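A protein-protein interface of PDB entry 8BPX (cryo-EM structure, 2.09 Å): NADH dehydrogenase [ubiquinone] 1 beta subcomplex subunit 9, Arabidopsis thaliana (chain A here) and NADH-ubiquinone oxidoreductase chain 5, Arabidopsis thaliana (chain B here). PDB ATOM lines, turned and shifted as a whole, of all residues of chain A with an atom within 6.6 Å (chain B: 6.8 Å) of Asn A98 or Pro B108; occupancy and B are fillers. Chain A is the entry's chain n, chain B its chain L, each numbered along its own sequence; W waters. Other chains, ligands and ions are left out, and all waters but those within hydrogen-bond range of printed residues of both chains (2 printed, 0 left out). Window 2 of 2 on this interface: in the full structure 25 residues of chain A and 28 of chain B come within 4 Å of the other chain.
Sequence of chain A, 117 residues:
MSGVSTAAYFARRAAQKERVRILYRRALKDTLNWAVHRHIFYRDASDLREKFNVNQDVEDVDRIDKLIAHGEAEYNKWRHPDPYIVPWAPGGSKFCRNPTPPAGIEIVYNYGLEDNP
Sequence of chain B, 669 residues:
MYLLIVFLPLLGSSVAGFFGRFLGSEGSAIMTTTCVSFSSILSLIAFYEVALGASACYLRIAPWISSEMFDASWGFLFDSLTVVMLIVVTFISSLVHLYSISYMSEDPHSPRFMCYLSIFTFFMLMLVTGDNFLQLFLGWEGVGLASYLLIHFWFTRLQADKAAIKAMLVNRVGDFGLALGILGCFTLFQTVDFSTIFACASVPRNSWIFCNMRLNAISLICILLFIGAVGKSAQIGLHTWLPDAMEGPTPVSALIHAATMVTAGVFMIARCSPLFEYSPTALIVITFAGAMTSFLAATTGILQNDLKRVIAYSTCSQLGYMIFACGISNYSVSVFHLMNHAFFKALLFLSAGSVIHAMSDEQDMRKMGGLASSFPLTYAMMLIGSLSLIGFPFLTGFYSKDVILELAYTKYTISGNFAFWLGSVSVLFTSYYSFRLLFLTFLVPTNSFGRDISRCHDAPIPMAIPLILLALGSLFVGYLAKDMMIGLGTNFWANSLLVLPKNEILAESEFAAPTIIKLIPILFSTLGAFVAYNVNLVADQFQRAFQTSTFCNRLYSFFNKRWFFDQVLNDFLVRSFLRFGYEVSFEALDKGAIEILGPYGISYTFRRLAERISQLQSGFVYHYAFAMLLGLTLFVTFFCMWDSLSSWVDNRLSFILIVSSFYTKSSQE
ND2 of Asn A98 lies within hydrogen-bond range of OD2 of Asp B107 (3.3 Å). The side-chain hydroxyl (OG1) of Thr B156 sits at hydrogen-bond distance from the backbone carbonyl oxygen (O) of Cys A96.
Hydrophobic or aromatic side chains of chain A that line the printed part of chain B: Pro A99. Along chain A the printed residues that touch a printed residue of chain B span positions 96 to 99. Hydrophobic or aromatic side chains of chain B within 4 Å of the printed part of chain A: Pro B108 and Trp B154. Among the printed residues, 6 pairs touch across the chains. Among the printed residues, no Asp or Glu carboxylate lies within 4 Å of a Lys or Arg side-chain nitrogen of the other chain.
Trp B154 touches Arg A97. ND2 of Asn A98 touches CD of Pro B108, 3.5 Å away. CD1 of Trp B154 touches OD1 of Asn A98, 3.6 Å away. Pro A99 touches Thr B156 (CD to OG1, 3.4 Å).
Water W1 lies within hydrogen-bond range of the side-chain hydroxyl (OG1) of Thr B156 (2.6 Å) and the backbone NH (N) of Asn A98 (3.2 Å). Water W2 lies within hydrogen-bond range of OD1 of Asp B107 (2.7 Å), OD1 of Asn A98 (2.8 Å) and ND1 of His B109 (2.8 Å).
N of His B109 sits at hydrogen-bond distance from OD1 of Asp B107, 2.7 Å away. The side-chain carboxylate (OD2) of Asp B107 lies within hydrogen-bond range of the indole nitrogen (NE1) of Trp B154 (3.0 Å).
Asn A98 touches just these residues of chain B: Asp B107, Pro B108 and Trp B154. Of chain A, only Asn A98 (3.5 Å) comes within 4 Å of Pro B108. Of the printed residues of chain B, Pro A99 touches Thr B156 (3.4 Å). Of the printed residues of chain B, Cys A96 touches Thr B156. Glu B106 touches none of the printed residues of chain A. Phe B153 touches none of the printed residues of chain A. The nearest residue of chain B that does not touch Asn A98 is Thr B156 (4.3 Å). The nearest printed residue of chain A that does not touch Pro B108 is Pro A99 (7.2 Å). The nearest printed residue of chain B that does not touch Pro A99 is Trp B154 (7.2 Å).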
ATOM      1  N   LYS A  94      -2.353  14.924 -25.867  1.00  0.00           N
ATOM      2  CA  LYS A  94      -2.695  16.305 -25.541  1.00  0.00           C
ATOM      3  C   LYS A  94      -3.936  16.434 -24.662  1.00  0.00           C
ATOM      4  O   LYS A  94      -4.361  17.556 -24.375  1.00  0.00           O
ATOM      5  CB  LYS A  94      -2.900  17.114 -26.821  1.00  0.00           C
ATOM      6  CG  LYS A  94      -2.104  18.391 -26.882  1.00  0.00           C
ATOM      7  CD  LYS A  94      -2.790  19.401 -27.772  1.00  0.00           C
ATOM      8  CE  LYS A  94      -1.907  20.592 -28.047  1.00  0.00           C
ATOM      9  NZ  LYS A  94      -2.387  21.372 -29.215  1.00  0.00           N
ATOM     10  N   CYS A  96      -6.466  17.023 -21.866  1.00  0.00           N
ATOM     11  CA  CYS A  96      -6.492  17.750 -20.590  1.00  0.00           C
ATOM     12  C   CYS A  96      -5.219  18.560 -20.335  1.00  0.00           C
ATOM     13  O   CYS A  96      -4.854  18.787 -19.180  1.00  0.00           O
ATOM     14  CB  CYS A  96      -6.750  16.805 -19.411  1.00  0.00           C
ATOM     15  SG  CYS A  96      -8.172  15.706 -19.584  1.00  0.00           S
ATOM     16  N   ARG A  97      -4.590  18.960 -21.432  1.00  0.00           N
ATOM     17  CA  ARG A  97      -3.509  19.930 -21.376  1.00  0.00           C
ATOM     18  C   ARG A  97      -4.106  21.320 -21.597  1.00  0.00           C
ATOM     19  O   ARG A  97      -4.862  21.458 -22.496  1.00  0.00           O
ATOM     20  CB  ARG A  97      -2.478  19.681 -22.472  1.00  0.00           C
ATOM     21  CG  ARG A  97      -1.230  20.541 -22.330  1.00  0.00           C
ATOM     22  CD  ARG A  97      -0.385  20.612 -23.583  1.00  0.00           C
ATOM     23  NE  ARG A  97       0.288  19.356 -23.843  1.00  0.00           N
ATOM     24  CZ  ARG A  97       0.991  19.067 -24.929  1.00  0.00           C
ATOM     25  NH1 ARG A  97       1.124  19.958 -25.894  1.00  0.00           N
ATOM     26  NH2 ARG A  97       1.559  17.886 -25.039  1.00  0.00           N
ATOM     27  N   ASN A  98      -3.780  22.266 -20.749  1.00  0.00           N
ATOM     28  CA  ASN A  98      -4.295  23.657 -20.823  1.00  0.00           C
ATOM     29  C   ASN A  98      -5.817  23.696 -21.096  1.00  0.00           C
ATOM     30  O   ASN A  98      -6.214  24.361 -21.986  1.00  0.00           O
ATOM     31  CB  ASN A  98      -3.403  24.512 -21.719  1.00  0.00           C
ATOM     32  CG  ASN A  98      -1.949  24.479 -21.313  1.00  0.00           C
ATOM     33  OD1 ASN A  98      -1.634  24.501 -20.133  1.00  0.00           O
ATOM     34  ND2 ASN A  98      -1.062  24.418 -22.283  1.00  0.00           N
ATOM     35  N   PRO A  99      -6.653  23.004 -20.318  1.00  0.00           N
ATOM     36  CA  PRO A  99      -8.100  23.091 -20.530  1.00  0.00           C
ATOM     37  C   PRO A  99      -8.629  24.481 -20.236  1.00  0.00           C
ATOM     38  O   PRO A  99      -8.056  25.241 -19.453  1.00  0.00           O
ATOM     39  CB  PRO A  99      -8.660  22.068 -19.540  1.00  0.00           C
ATOM     40  CG  PRO A  99      -7.659  22.050 -18.435  1.00  0.00           C
ATOM     41  CD  PRO A  99      -6.317  22.295 -19.070  1.00  0.00           C
ATOM     42  N   THR A 100      -9.735  24.807 -20.886  1.00  0.00           N
ATOM     43  CA  THR A 100     -10.448  26.017 -20.529  1.00  0.00           C
ATOM     44  C   THR A 100     -10.968  25.887 -19.100  1.00  0.00           C
ATOM     45  O   THR A 100     -11.397  24.803 -18.692  1.00  0.00           O
ATOM     46  CB  THR A 100     -11.605  26.278 -21.496  1.00  0.00           C
ATOM     47  OG1 THR A 100     -11.088  26.448 -22.822  1.00  0.00           O
ATOM     48  CG2 THR A 100     -12.363  27.522 -21.099  1.00  0.00           C
ATOM     49  N   PRO A 101     -10.917  26.956 -18.309  1.00  0.00           N
ATOM     50  CA  PRO A 101     -11.361  26.855 -16.925  1.00  0.00           C
ATOM     51  C   PRO A 101     -12.848  26.574 -16.858  1.00  0.00           C
ATOM     52  O   PRO A 101     -13.618  26.977 -17.750  1.00  0.00           O
ATOM     53  CB  PRO A 101     -11.024  28.236 -16.344  1.00  0.00           C
ATOM     54  CG  PRO A 101     -10.110  28.874 -17.306  1.00  0.00           C
ATOM     55  CD  PRO A 101     -10.382  28.285 -18.640  1.00  0.00           C
ATOM     56  N   SER B  25       6.003  36.533 -19.379  1.00  0.00           N
ATOM     57  CA  SER B  25       6.646  35.486 -20.165  1.00  0.00           C
ATOM     58  C   SER B  25       7.990  35.953 -20.698  1.00  0.00           C
ATOM     59  O   SER B  25       9.018  35.288 -20.509  1.00  0.00           O
ATOM     60  CB  SER B  25       5.732  35.077 -21.318  1.00  0.00           C
ATOM     61  OG  SER B  25       4.448  34.739 -20.849  1.00  0.00           O
ATOM     62  N   MET B 104       7.664  27.036 -25.846  1.00  0.00           N
ATOM     63  CA  MET B 104       6.583  27.252 -24.896  1.00  0.00           C
ATOM     64  C   MET B 104       5.943  28.622 -25.067  1.00  0.00           C
ATOM     65  O   MET B 104       5.266  29.105 -24.154  1.00  0.00           O
ATOM     66  CB  MET B 104       7.102  27.085 -23.468  1.00  0.00           C
ATOM     67  CG  MET B 104       7.648  25.695 -23.153  1.00  0.00           C
ATOM     68  SD  MET B 104       6.373  24.431 -22.992  1.00  0.00           S
ATOM     69  CE  MET B 104       5.782  24.755 -21.330  1.00  0.00           C
ATOM     70  N   SER B 105       6.141  29.254 -26.227  1.00  0.00           N
ATOM     71  CA  SER B 105       5.715  30.635 -26.415  1.00  0.00           C
ATOM     72  C   SER B 105       4.202  30.784 -26.337  1.00  0.00           C
ATOM     73  O   SER B 105       3.706  31.830 -25.907  1.00  0.00           O
ATOM     74  CB  SER B 105       6.233  31.160 -27.753  1.00  0.00           C
ATOM     75  OG  SER B 105       5.429  30.708 -28.822  1.00  0.00           O
ATOM     76  N   GLU B 106       3.453  29.764 -26.741  1.00  0.00           N
ATOM     77  CA  GLU B 106       2.002  29.806 -26.645  1.00  0.00           C
ATOM     78  C   GLU B 106       1.465  29.188 -25.357  1.00  0.00           C
ATOM     79  O   GLU B 106       0.249  29.195 -25.148  1.00  0.00           O
ATOM     80  CB  GLU B 106       1.367  29.106 -27.848  1.00  0.00           C
ATOM     81  CG  GLU B 106       1.251  29.966 -29.092  1.00  0.00           C
ATOM     82  CD  GLU B 106       2.589  30.428 -29.622  1.00  0.00           C
ATOM     83  OE1 GLU B 106       3.455  29.569 -29.890  1.00  0.00           O
ATOM     84  OE2 GLU B 106       2.782  31.655 -29.762  1.00  0.00           O
ATOM     85  N   ASP B 107       2.326  28.648 -24.504  1.00  0.00           N
ATOM     86  CA  ASP B 107       1.855  28.068 -23.254  1.00  0.00           C
ATOM     87  C   ASP B 107       1.450  29.168 -22.276  1.00  0.00           C
ATOM     88  O   ASP B 107       2.114  30.203 -22.195  1.00  0.00           O
ATOM     89  CB  ASP B 107       2.926  27.175 -22.629  1.00  0.00           C
ATOM     90  CG  ASP B 107       2.405  26.384 -21.437  1.00  0.00           C
ATOM     91  OD1 ASP B 107       2.266  26.966 -20.345  1.00  0.00           O
ATOM     92  OD2 ASP B 107       2.098  25.190 -21.605  1.00  0.00           O
ATOM     93  N   PRO B 108       0.363  28.972 -21.526  1.00  0.00           N
ATOM     94  CA  PRO B 108      -0.062  30.008 -20.571  1.00  0.00           C
ATOM     95  C   PRO B 108       0.911  30.246 -19.424  1.00  0.00           C
ATOM     96  O   PRO B 108       0.926  31.352 -18.877  1.00  0.00           O
ATOM     97  CB  PRO B 108      -1.409  29.481 -20.053  1.00  0.00           C
ATOM     98  CG  PRO B 108      -1.837  28.451 -21.026  1.00  0.00           C
ATOM     99  CD  PRO B 108      -0.599  27.861 -21.608  1.00  0.00           C
ATOM    100  N   HIS B 109       1.610  29.214 -19.032  1.00  0.00           N
ATOM    101  CA  HIS B 109       2.440  29.315 -17.812  1.00  0.00           C
ATOM    102  C   HIS B 109       3.977  29.276 -18.028  1.00  0.00           C
ATOM    103  O   HIS B 109       4.658  28.721 -17.168  1.00  0.00           O
ATOM    104  CB  HIS B 109       1.906  28.283 -16.815  1.00  0.00           C
ATOM    105  CG  HIS B 109       0.461  28.430 -16.528  1.00  0.00           C
ATOM    106  ND1 HIS B 109      -0.467  27.537 -17.002  1.00  0.00           N
ATOM    107  CD2 HIS B 109      -0.226  29.388 -15.881  1.00  0.00           C
ATOM    108  CE1 HIS B 109      -1.654  27.904 -16.611  1.00  0.00           C
ATOM    109  NE2 HIS B 109      -1.534  29.034 -15.945  1.00  0.00           N
ATOM    110  N   SER B 110       4.507  29.916 -19.036  1.00  0.00           N
ATOM    111  CA  SER B 110       5.940  29.840 -19.323  1.00  0.00           C
ATOM    112  C   SER B 110       6.849  30.325 -18.189  1.00  0.00           C
ATOM    113  O   SER B 110       7.921  29.722 -18.012  1.00  0.00           O
ATOM    114  CB  SER B 110       6.244  30.578 -20.635  1.00  0.00           C
ATOM    115  OG  SER B 110       6.164  31.981 -20.497  1.00  0.00           O
ATOM    116  N   PRO B 111       6.537  31.390 -17.429  1.00  0.00           N
ATOM    117  CA  PRO B 111       7.463  31.786 -16.350  1.00  0.00           C
ATOM    118  C   PRO B 111       7.708  30.704 -15.306  1.00  0.00           C
ATOM    119  O   PRO B 111       8.858  30.506 -14.886  1.00  0.00           O
ATOM    120  CB  PRO B 111       6.780  33.022 -15.744  1.00  0.00           C
ATOM    121  CG  PRO B 111       5.925  33.541 -16.826  1.00  0.00           C
ATOM    122  CD  PRO B 111       5.416  32.342 -17.538  1.00  0.00           C
ATOM    123  N   PHE B 153       4.127  19.235 -15.057  1.00  0.00           N
ATOM    124  CA  PHE B 153       3.969  20.668 -15.291  1.00  0.00           C
ATOM    125  C   PHE B 153       2.554  21.018 -15.737  1.00  0.00           C
ATOM    126  O   PHE B 153       1.992  22.028 -15.302  1.00  0.00           O
ATOM    127  CB  PHE B 153       4.981  21.143 -16.337  1.00  0.00           C
ATOM    128  CG  PHE B 153       4.769  22.561 -16.780  1.00  0.00           C
ATOM    129  CD1 PHE B 153       5.167  23.616 -15.978  1.00  0.00           C
ATOM    130  CD2 PHE B 153       4.149  22.840 -17.986  1.00  0.00           C
ATOM    131  CE1 PHE B 153       4.964  24.923 -16.374  1.00  0.00           C
ATOM    132  CE2 PHE B 153       3.940  24.144 -18.388  1.00  0.00           C
ATOM    133  CZ  PHE B 153       4.353  25.186 -17.581  1.00  0.00           C
ATOM    134  N   TRP B 154       1.989  20.245 -16.648  1.00  0.00           N
ATOM    135  CA  TRP B 154       0.552  20.306 -17.031  1.00  0.00           C
ATOM    136  C   TRP B 154      -0.268  19.567 -15.937  1.00  0.00           C
ATOM    137  O   TRP B 154      -0.664  18.433 -16.158  1.00  0.00           O
ATOM    138  CB  TRP B 154       0.348  19.783 -18.442  1.00  0.00           C
ATOM    139  CG  TRP B 154       0.985  20.644 -19.487  1.00  0.00           C
ATOM    140  CD1 TRP B 154       0.870  21.996 -19.621  1.00  0.00           C
ATOM    141  CD2 TRP B 154       1.854  20.208 -20.546  1.00  0.00           C
ATOM    142  NE1 TRP B 154       1.577  22.426 -20.706  1.00  0.00           N
ATOM    143  CE2 TRP B 154       2.193  21.354 -21.294  1.00  0.00           C
ATOM    144  CE3 TRP B 154       2.357  18.966 -20.942  1.00  0.00           C
ATOM    145  CZ2 TRP B 154       3.022  21.291 -22.410  1.00  0.00           C
ATOM    146  CZ3 TRP B 154       3.181  18.904 -22.046  1.00  0.00           C
ATOM    147  CH2 TRP B 154       3.507  20.053 -22.764  1.00  0.00           C
ATOM    148  N   THR B 156      -3.212  19.427 -14.768  1.00  0.00           N
ATOM    149  CA  THR B 156      -4.605  18.972 -15.025  1.00  0.00           C
ATOM    150  C   THR B 156      -4.614  17.574 -15.657  1.00  0.00           C
ATOM    151  O   THR B 156      -5.631  17.002 -15.695  1.00  0.00           O
ATOM    152  CB  THR B 156      -5.344  20.099 -15.778  1.00  0.00           C
ATOM    153  OG1 THR B 156      -4.616  20.264 -16.993  1.00  0.00           O
ATOM    154  CG2 THR B 156      -5.418  21.409 -15.033  1.00  0.00           C
HETATM  155  O   HOH W   1      -2.497  21.420 -17.947  1.00  0.00           O
HETATM  156  O   HOH W   2       0.509  25.609 -18.760  1.00  0.00           O
